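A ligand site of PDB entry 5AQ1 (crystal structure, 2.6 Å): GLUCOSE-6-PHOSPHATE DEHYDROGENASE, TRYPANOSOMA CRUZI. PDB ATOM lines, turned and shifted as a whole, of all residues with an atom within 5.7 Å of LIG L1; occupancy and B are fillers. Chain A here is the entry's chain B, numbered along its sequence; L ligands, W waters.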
ATOM      1  N   LYS A 181      23.842 -25.439 -10.873  1.00  0.00           N
ATOM      2  CA  LYS A 181      24.820 -26.399 -11.375  1.00  0.00           C
ATOM      3  C   LYS A 181      26.063 -25.631 -11.847  1.00  0.00           C
ATOM      4  O   LYS A 181      25.973 -24.421 -12.049  1.00  0.00           O
ATOM      5  CB  LYS A 181      24.208 -27.244 -12.504  1.00  0.00           C
ATOM      6  CG  LYS A 181      24.074 -26.557 -13.855  1.00  0.00           C
ATOM      7  CD  LYS A 181      23.351 -27.458 -14.848  1.00  0.00           C
ATOM      8  CE  LYS A 181      23.173 -26.809 -16.211  1.00  0.00           C
ATOM      9  NZ  LYS A 181      24.396 -26.885 -17.053  1.00  0.00           N
ATOM     10  N   HIS A 211      16.805 -25.866 -14.452  1.00  0.00           N
ATOM     11  CA  HIS A 211      15.832 -24.879 -14.918  1.00  0.00           C
ATOM     12  C   HIS A 211      14.886 -25.401 -16.002  1.00  0.00           C
ATOM     13  O   HIS A 211      13.856 -24.783 -16.262  1.00  0.00           O
ATOM     14  CB  HIS A 211      16.514 -23.562 -15.330  1.00  0.00           C
ATOM     15  CG  HIS A 211      16.972 -23.508 -16.745  1.00  0.00           C
ATOM     16  ND1 HIS A 211      18.205 -23.983 -17.153  1.00  0.00           N
ATOM     17  CD2 HIS A 211      16.378 -23.007 -17.858  1.00  0.00           C
ATOM     18  CE1 HIS A 211      18.336 -23.797 -18.449  1.00  0.00           C
ATOM     19  NE2 HIS A 211      17.245 -23.206 -18.907  1.00  0.00           N
ATOM     20  N   TYR A 212      15.221 -26.536 -16.597  1.00  0.00           N
ATOM     21  CA  TYR A 212      14.299 -27.175 -17.546  1.00  0.00           C
ATOM     22  C   TYR A 212      12.984 -27.610 -16.896  1.00  0.00           C
ATOM     23  O   TYR A 212      11.952 -27.666 -17.562  1.00  0.00           O
ATOM     24  CB  TYR A 212      14.995 -28.342 -18.263  1.00  0.00           C
ATOM     25  CG  TYR A 212      15.720 -27.902 -19.528  1.00  0.00           C
ATOM     26  CD1 TYR A 212      16.446 -26.714 -19.560  1.00  0.00           C
ATOM     27  CD2 TYR A 212      15.663 -28.672 -20.678  1.00  0.00           C
ATOM     28  CE1 TYR A 212      17.100 -26.304 -20.706  1.00  0.00           C
ATOM     29  CE2 TYR A 212      16.322 -28.272 -21.830  1.00  0.00           C
ATOM     30  CZ  TYR A 212      17.029 -27.088 -21.834  1.00  0.00           C
ATOM     31  OH  TYR A 212      17.679 -26.687 -22.982  1.00  0.00           O
ATOM     32  N   LYS A 215      10.041 -25.155 -17.417  1.00  0.00           N
ATOM     33  CA  LYS A 215       9.511 -24.934 -18.763  1.00  0.00           C
ATOM     34  C   LYS A 215       8.133 -25.546 -18.902  1.00  0.00           C
ATOM     35  O   LYS A 215       7.895 -26.667 -18.449  1.00  0.00           O
ATOM     36  CB  LYS A 215      10.457 -25.515 -19.816  1.00  0.00           C
ATOM     37  CG  LYS A 215      11.799 -24.803 -19.910  1.00  0.00           C
ATOM     38  CD  LYS A 215      12.572 -25.218 -21.147  1.00  0.00           C
ATOM     39  CE  LYS A 215      13.968 -24.602 -21.165  1.00  0.00           C
ATOM     40  NZ  LYS A 215      13.942 -23.133 -21.380  1.00  0.00           N
ATOM     41  N   PHE A 247      18.024 -32.211 -27.939  1.00  0.00           N
ATOM     42  CA  PHE A 247      18.440 -30.855 -27.611  1.00  0.00           C
ATOM     43  C   PHE A 247      19.338 -30.360 -28.733  1.00  0.00           C
ATOM     44  O   PHE A 247      20.335 -30.997 -29.074  1.00  0.00           O
ATOM     45  CB  PHE A 247      19.188 -30.843 -26.270  1.00  0.00           C
ATOM     46  CG  PHE A 247      19.921 -29.569 -25.976  1.00  0.00           C
ATOM     47  CD1 PHE A 247      21.232 -29.390 -26.412  1.00  0.00           C
ATOM     48  CD2 PHE A 247      19.327 -28.561 -25.231  1.00  0.00           C
ATOM     49  CE1 PHE A 247      21.921 -28.218 -26.135  1.00  0.00           C
ATOM     50  CE2 PHE A 247      20.019 -27.380 -24.950  1.00  0.00           C
ATOM     51  CZ  PHE A 247      21.312 -27.215 -25.397  1.00  0.00           C
ATOM     52  N   GLU A 249      21.082 -26.543 -30.422  1.00  0.00           N
ATOM     53  CA  GLU A 249      21.310 -25.097 -30.364  1.00  0.00           C
ATOM     54  C   GLU A 249      22.100 -24.670 -31.579  1.00  0.00           C
ATOM     55  O   GLU A 249      22.924 -25.442 -32.087  1.00  0.00           O
ATOM     56  CB  GLU A 249      22.075 -24.715 -29.096  1.00  0.00           C
ATOM     57  CG  GLU A 249      21.191 -24.517 -27.867  1.00  0.00           C
ATOM     58  CD  GLU A 249      21.988 -24.172 -26.616  1.00  0.00           C
ATOM     59  OE1 GLU A 249      23.235 -24.263 -26.648  1.00  0.00           O
ATOM     60  OE2 GLU A 249      21.374 -23.796 -25.600  1.00  0.00           O
ATOM     61  N   ILE A 251      23.835 -21.724 -31.372  1.00  0.00           N
ATOM     62  CA  ILE A 251      25.002 -21.109 -30.729  1.00  0.00           C
ATOM     63  C   ILE A 251      26.119 -22.125 -30.496  1.00  0.00           C
ATOM     64  O   ILE A 251      25.860 -23.317 -30.335  1.00  0.00           O
ATOM     65  CB  ILE A 251      24.656 -20.413 -29.395  1.00  0.00           C
ATOM     66  CG1 ILE A 251      23.995 -21.392 -28.408  1.00  0.00           C
ATOM     67  CG2 ILE A 251      23.747 -19.213 -29.639  1.00  0.00           C
ATOM     68  CD1 ILE A 251      24.053 -20.915 -26.971  1.00  0.00           C
ATOM     69  N   PHE A 260      33.627 -24.390 -21.065  1.00  0.00           N
ATOM     70  CA  PHE A 260      32.945 -25.578 -21.563  1.00  0.00           C
ATOM     71  C   PHE A 260      33.887 -26.782 -21.730  1.00  0.00           C
ATOM     72  O   PHE A 260      33.448 -27.925 -21.591  1.00  0.00           O
ATOM     73  CB  PHE A 260      32.267 -25.262 -22.901  1.00  0.00           C
ATOM     74  CG  PHE A 260      31.370 -26.345 -23.394  1.00  0.00           C
ATOM     75  CD1 PHE A 260      30.032 -26.401 -23.008  1.00  0.00           C
ATOM     76  CD2 PHE A 260      31.845 -27.320 -24.264  1.00  0.00           C
ATOM     77  CE1 PHE A 260      29.191 -27.400 -23.474  1.00  0.00           C
ATOM     78  CE2 PHE A 260      31.014 -28.321 -24.735  1.00  0.00           C
ATOM     79  CZ  PHE A 260      29.684 -28.362 -24.334  1.00  0.00           C
ATOM     80  N   ASP A 268      26.957 -30.872 -19.375  1.00  0.00           N
ATOM     81  CA  ASP A 268      26.294 -29.576 -19.499  1.00  0.00           C
ATOM     82  C   ASP A 268      24.768 -29.659 -19.587  1.00  0.00           C
ATOM     83  O   ASP A 268      24.072 -28.891 -18.921  1.00  0.00           O
ATOM     84  CB  ASP A 268      26.836 -28.822 -20.726  1.00  0.00           C
ATOM     85  CG  ASP A 268      26.406 -27.351 -20.758  1.00  0.00           C
ATOM     86  OD1 ASP A 268      26.438 -26.684 -19.702  1.00  0.00           O
ATOM     87  OD2 ASP A 268      26.052 -26.873 -21.848  1.00  0.00           O
ATOM     88  N   VAL A 269      24.259 -30.599 -20.390  1.00  0.00           N
ATOM     89  CA  VAL A 269      22.795 -30.715 -20.599  1.00  0.00           C
ATOM     90  C   VAL A 269      22.204 -32.117 -20.471  1.00  0.00           C
ATOM     91  O   VAL A 269      21.038 -32.252 -20.095  1.00  0.00           O
ATOM     92  CB  VAL A 269      22.367 -30.125 -21.959  1.00  0.00           C
ATOM     93  CG1 VAL A 269      22.850 -28.678 -22.095  1.00  0.00           C
ATOM     94  CG2 VAL A 269      22.886 -30.951 -23.117  1.00  0.00           C
ATOM     95  N   ASN A 272      21.803 -33.562 -16.640  1.00  0.00           N
ATOM     96  CA  ASN A 272      20.824 -32.828 -15.854  1.00  0.00           C
ATOM     97  C   ASN A 272      19.511 -32.620 -16.606  1.00  0.00           C
ATOM     98  O   ASN A 272      18.510 -33.274 -16.295  1.00  0.00           O
ATOM     99  CB  ASN A 272      21.415 -31.502 -15.329  1.00  0.00           C
ATOM    100  CG  ASN A 272      22.296 -30.805 -16.353  1.00  0.00           C
ATOM    101  OD1 ASN A 272      21.805 -30.263 -17.350  1.00  0.00           O
ATOM    102  ND2 ASN A 272      23.603 -30.807 -16.113  1.00  0.00           N
ATOM    103  N   HIS A 273      19.500 -31.737 -17.603  1.00  0.00           N
ATOM    104  CA  HIS A 273      18.245 -31.332 -18.242  1.00  0.00           C
ATOM    105  C   HIS A 273      17.497 -32.515 -18.863  1.00  0.00           C
ATOM    106  O   HIS A 273      16.314 -32.716 -18.603  1.00  0.00           O
ATOM    107  CB  HIS A 273      18.505 -30.280 -19.329  1.00  0.00           C
ATOM    108  CG  HIS A 273      19.132 -29.023 -18.825  1.00  0.00           C
ATOM    109  ND1 HIS A 273      18.674 -28.368 -17.699  1.00  0.00           N
ATOM    110  CD2 HIS A 273      20.162 -28.281 -19.295  1.00  0.00           C
ATOM    111  CE1 HIS A 273      19.404 -27.281 -17.499  1.00  0.00           C
ATOM    112  NE2 HIS A 273      20.310 -27.206 -18.451  1.00  0.00           N
ATOM    113  N   LYS A 367      25.471 -28.550 -29.688  1.00  0.00           N
ATOM    114  CA  LYS A 367      25.581 -27.129 -29.978  1.00  0.00           C
ATOM    115  C   LYS A 367      26.143 -26.975 -31.389  1.00  0.00           C
ATOM    116  O   LYS A 367      26.648 -27.944 -31.977  1.00  0.00           O
ATOM    117  CB  LYS A 367      26.481 -26.446 -28.944  1.00  0.00           C
ATOM    118  CG  LYS A 367      25.855 -26.331 -27.561  1.00  0.00           C
ATOM    119  CD  LYS A 367      26.801 -25.683 -26.561  1.00  0.00           C
ATOM    120  CE  LYS A 367      26.179 -25.585 -25.164  1.00  0.00           C
ATOM    121  NZ  LYS A 367      25.348 -24.365 -24.977  1.00  0.00           N
ATOM    122  N   ARG A 372      17.611 -24.364 -33.224  1.00  0.00           N
ATOM    123  CA  ARG A 372      17.366 -24.440 -31.798  1.00  0.00           C
ATOM    124  C   ARG A 372      16.130 -25.307 -31.595  1.00  0.00           C
ATOM    125  O   ARG A 372      15.078 -25.045 -32.181  1.00  0.00           O
ATOM    126  CB  ARG A 372      17.125 -23.053 -31.221  1.00  0.00           C
ATOM    127  CG  ARG A 372      16.786 -23.046 -29.733  1.00  0.00           C
ATOM    128  CD  ARG A 372      17.203 -21.749 -29.070  1.00  0.00           C
ATOM    129  NE  ARG A 372      16.891 -21.751 -27.643  1.00  0.00           N
ATOM    130  CZ  ARG A 372      15.705 -21.429 -27.112  1.00  0.00           C
ATOM    131  NH1 ARG A 372      14.689 -21.041 -27.877  1.00  0.00           N
ATOM    132  NH2 ARG A 372      15.549 -21.474 -25.790  1.00  0.00           N
ATOM    133  N   GLN A 401      10.468 -26.037 -26.882  1.00  0.00           N
ATOM    134  CA  GLN A 401      10.892 -24.802 -27.543  1.00  0.00           C
ATOM    135  C   GLN A 401      11.534 -25.102 -28.910  1.00  0.00           C
ATOM    136  O   GLN A 401      12.113 -26.176 -29.084  1.00  0.00           O
ATOM    137  CB  GLN A 401      11.897 -24.043 -26.667  1.00  0.00           C
ATOM    138  CG  GLN A 401      13.278 -24.686 -26.603  1.00  0.00           C
ATOM    139  CD  GLN A 401      14.029 -24.382 -25.319  1.00  0.00           C
ATOM    140  OE1 GLN A 401      13.486 -23.804 -24.379  1.00  0.00           O
ATOM    141  NE2 GLN A 401      15.300 -24.765 -25.282  1.00  0.00           N
HETATM  142  C1  LIG L   1      22.357 -24.231 -19.485  1.00  0.00           C
HETATM  143  C2  LIG L   1      23.600 -24.841 -20.120  1.00  0.00           C
HETATM  144  O1  LIG L   1      22.009 -24.934 -18.288  1.00  0.00           O
HETATM  145  O2  LIG L   1      21.263 -24.306 -20.402  1.00  0.00           O
HETATM  146  C3  LIG L   1      23.913 -24.125 -21.425  1.00  0.00           C
HETATM  147  O3  LIG L   1      24.720 -24.745 -19.226  1.00  0.00           O
HETATM  148  C4  LIG L   1      22.689 -24.209 -22.331  1.00  0.00           C
HETATM  149  O4  LIG L   1      25.050 -24.697 -22.084  1.00  0.00           O
HETATM  150  C5  LIG L   1      21.490 -23.591 -21.627  1.00  0.00           C
HETATM  151  O5  LIG L   1      22.963 -23.540 -23.560  1.00  0.00           O
HETATM  152  C6  LIG L   1      20.249 -23.635 -22.509  1.00  0.00           C
HETATM  153  O6  LIG L   1      19.094 -23.228 -21.766  1.00  0.00           O
HETATM  154  P1  LIG L   1      17.740 -22.848 -22.541  1.00  0.00           P
HETATM  155  O7  LIG L   1      17.426 -24.059 -23.392  1.00  0.00           O
HETATM  156  O8  LIG L   1      16.728 -22.632 -21.451  1.00  0.00           O
HETATM  157  O9  LIG L   1      18.101 -21.612 -23.316  1.00  0.00           O
HETATM  158  P1  LG2 L   2      29.583 -15.440 -13.437  1.00  0.00           P
HETATM  159  O1  LG2 L   2      30.884 -15.928 -14.030  1.00  0.00           O
HETATM  160  O2  LG2 L   2      28.822 -14.315 -14.112  1.00  0.00           O
HETATM  161  O3  LG2 L   2      29.881 -15.077 -11.901  1.00  0.00           O
HETATM  162  C1  LG2 L   2      28.821 -14.597 -11.069  1.00  0.00           C
HETATM  163  C2  LG2 L   2      29.344 -13.554 -10.097  1.00  0.00           C
HETATM  164  O4  LG2 L   2      30.172 -14.218  -9.125  1.00  0.00           O
HETATM  165  C3  LG2 L   2      30.207 -12.458 -10.726  1.00  0.00           C
HETATM  166  O5  LG2 L   2      29.472 -11.273 -11.045  1.00  0.00           O
HETATM  167  C4  LG2 L   2      31.247 -12.183  -9.673  1.00  0.00           C
HETATM  168  O6  LG2 L   2      30.802 -11.139  -8.807  1.00  0.00           O
HETATM  169  C5  LG2 L   2      31.369 -13.475  -8.891  1.00  0.00           C
HETATM  170  N1  LG2 L   2      32.583 -14.216  -9.307  1.00  0.00           N
HETATM  171  C6  LG2 L   2      32.944 -14.544 -10.575  1.00  0.00           C
HETATM  172  N2  LG2 L   2      34.125 -15.217 -10.574  1.00  0.00           N
HETATM  173  C7  LG2 L   2      34.528 -15.335  -9.294  1.00  0.00           C
HETATM  174  C8  LG2 L   2      35.667 -15.938  -8.582  1.00  0.00           C
HETATM  175  N3  LG2 L   2      36.649 -16.563  -9.273  1.00  0.00           N
HETATM  176  N4  LG2 L   2      35.701 -15.830  -7.230  1.00  0.00           N
HETATM  177  C9  LG2 L   2      34.735 -15.214  -6.526  1.00  0.00           C
HETATM  178  N5  LG2 L   2      33.666 -14.649  -7.121  1.00  0.00           N
HETATM  179  C10 LG2 L   2      33.502 -14.677  -8.466  1.00  0.00           C
HETATM  180  O7  LG2 L   2      28.595 -16.696 -13.203  1.00  0.00           O
HETATM  181  P2  LG2 L   2      27.148 -16.827 -13.903  1.00  0.00           P
HETATM  182  O8  LG2 L   2      26.238 -15.707 -13.449  1.00  0.00           O
HETATM  183  O9  LG2 L   2      27.362 -17.065 -15.376  1.00  0.00           O
HETATM  184  O10 LG2 L   2      26.606 -18.192 -13.242  1.00  0.00           O
HETATM  185  C11 LG2 L   2      26.313 -18.289 -11.842  1.00  0.00           C
HETATM  186  C12 LG2 L   2      26.025 -19.742 -11.495  1.00  0.00           C
HETATM  187  O11 LG2 L   2      24.894 -20.211 -12.250  1.00  0.00           O
HETATM  188  C13 LG2 L   2      27.190 -20.643 -11.847  1.00  0.00           C
HETATM  189  O12 LG2 L   2      27.379 -21.636 -10.841  1.00  0.00           O
HETATM  190  C14 LG2 L   2      26.789 -21.293 -13.157  1.00  0.00           C
HETATM  191  O13 LG2 L   2      27.403 -22.582 -13.337  1.00  0.00           O
HETATM  192  C15 LG2 L   2      25.266 -21.341 -13.056  1.00  0.00           C
HETATM  193  N6  LG2 L   2      24.629 -21.325 -14.381  1.00  0.00           N
HETATM  194  C16 LG2 L   2      24.486 -20.179 -15.069  1.00  0.00           C
HETATM  195  C17 LG2 L   2      23.895 -20.146 -16.323  1.00  0.00           C
HETATM  196  C18 LG2 L   2      23.738 -18.846 -17.064  1.00  0.00           C
HETATM  197  O14 LG2 L   2      22.752 -18.684 -17.768  1.00  0.00           O
HETATM  198  N7  LG2 L   2      24.672 -17.896 -16.959  1.00  0.00           N
HETATM  199  C19 LG2 L   2      23.380 -21.410 -16.967  1.00  0.00           C
HETATM  200  C20 LG2 L   2      23.592 -22.585 -16.122  1.00  0.00           C
HETATM  201  C21 LG2 L   2      24.195 -22.499 -14.877  1.00  0.00           C
HETATM  202  P3  LG2 L   2      31.786 -10.232  -7.926  1.00  0.00           P
HETATM  203  O15 LG2 L   2      33.142 -10.305  -8.599  1.00  0.00           O
HETATM  204  O16 LG2 L   2      31.130  -8.880  -8.027  1.00  0.00           O
HETATM  205  O17 LG2 L   2      31.764 -10.862  -6.546  1.00  0.00           O
HETATM  206  O   HOH W   1      20.726 -23.389 -16.157  1.00  0.00           O
HETATM  207  O   HOH W   2      18.585 -24.087 -25.795  1.00  0.00           O
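An oxygen (O4) of LIG L1 sits at hydrogen-bond distance from the side-chain carboxylate (OD2) of Asp 268 (2.4 Å). An oxygen (O5) of LIG L1 sits at hydrogen-bond distance from the side-chain carboxylate (OE2) of Glu 249 (2.6 Å). NE2 of His 211 lies within hydrogen-bond range of O8 of LIG L1 (2.7 Å). OH of Tyr 212 lies within hydrogen-bond range of O7 of LIG L1 (2.7 Å). An oxygen (O8) of LIG L1 lies within salt-bridge range of the side-chain amino group of Lys 215, at 2.8 Å. An oxygen (O1) of LIG L1 lies within hydrogen-bond range of a ring nitrogen (NE2) of His 273. The side-chain amino group (NZ) of Lys 367 is in hydrogen-bond range of an oxygen (O5) of LIG L1 (2.9 Å). An oxygen (O7) of LIG L1 sits at hydrogen-bond distance from the side-chain amide nitrogen (NE2) of Gln 401. The side-chain amino group (NZ) of Lys 181 sits at hydrogen-bond distance from an oxygen (O3) of LIG L1, 3.1 Å away. An oxygen (O9) of LIG L1 lies within salt-bridge range of the guanidinium group (NH2) of Arg 372 (3.6 Å). O13 of LG2 L2 is in hydrogen-bond range of O of Lys 181.
OD1 of Asp 268 is in salt-bridge range of NZ of Lys 181 (3.4 Å). The side-chain amide oxygen of Asn 272 lies close to the backbone carbonyl oxygen of Asp 268. The side-chain carboxylate (OE1) of Glu 249 lies within salt-bridge range of the side-chain amino group (NZ) of Lys 367 (2.7 Å). NZ of Lys 215 lies within hydrogen-bond range of OE1 of Gln 401, 3.1 Å away. The side-chain amide nitrogen (NE2) of Gln 401 sits close to the guanidinium group (NH2) of Arg 372 (3.3 Å).
Hydrophobic or aromatic side chains within 4 Å of LIG L1: His 211, Tyr 212 and His 273. Within 4 Å of LIG L1: Lys 181, His 211, Tyr 212, Lys 215, Glu 249, Asp 268, His 273, Lys 367, Arg 372 and Gln 401. The nearest printed residue that does not touch LIG L1 is Val 269 (4.4 Å).
Water W2 lies within hydrogen-bond range of O7 of LIG L1 (2.7 Å), OE2 of Glu 249 (2.8 Å), NE2 of Gln 401 (3.4 Å) and NE of Arg 372 (3.4 Å). Water W1 lies within hydrogen-bond range of a ring nitrogen (ND1) of His 211 and an oxygen (O1) of LIG L1.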
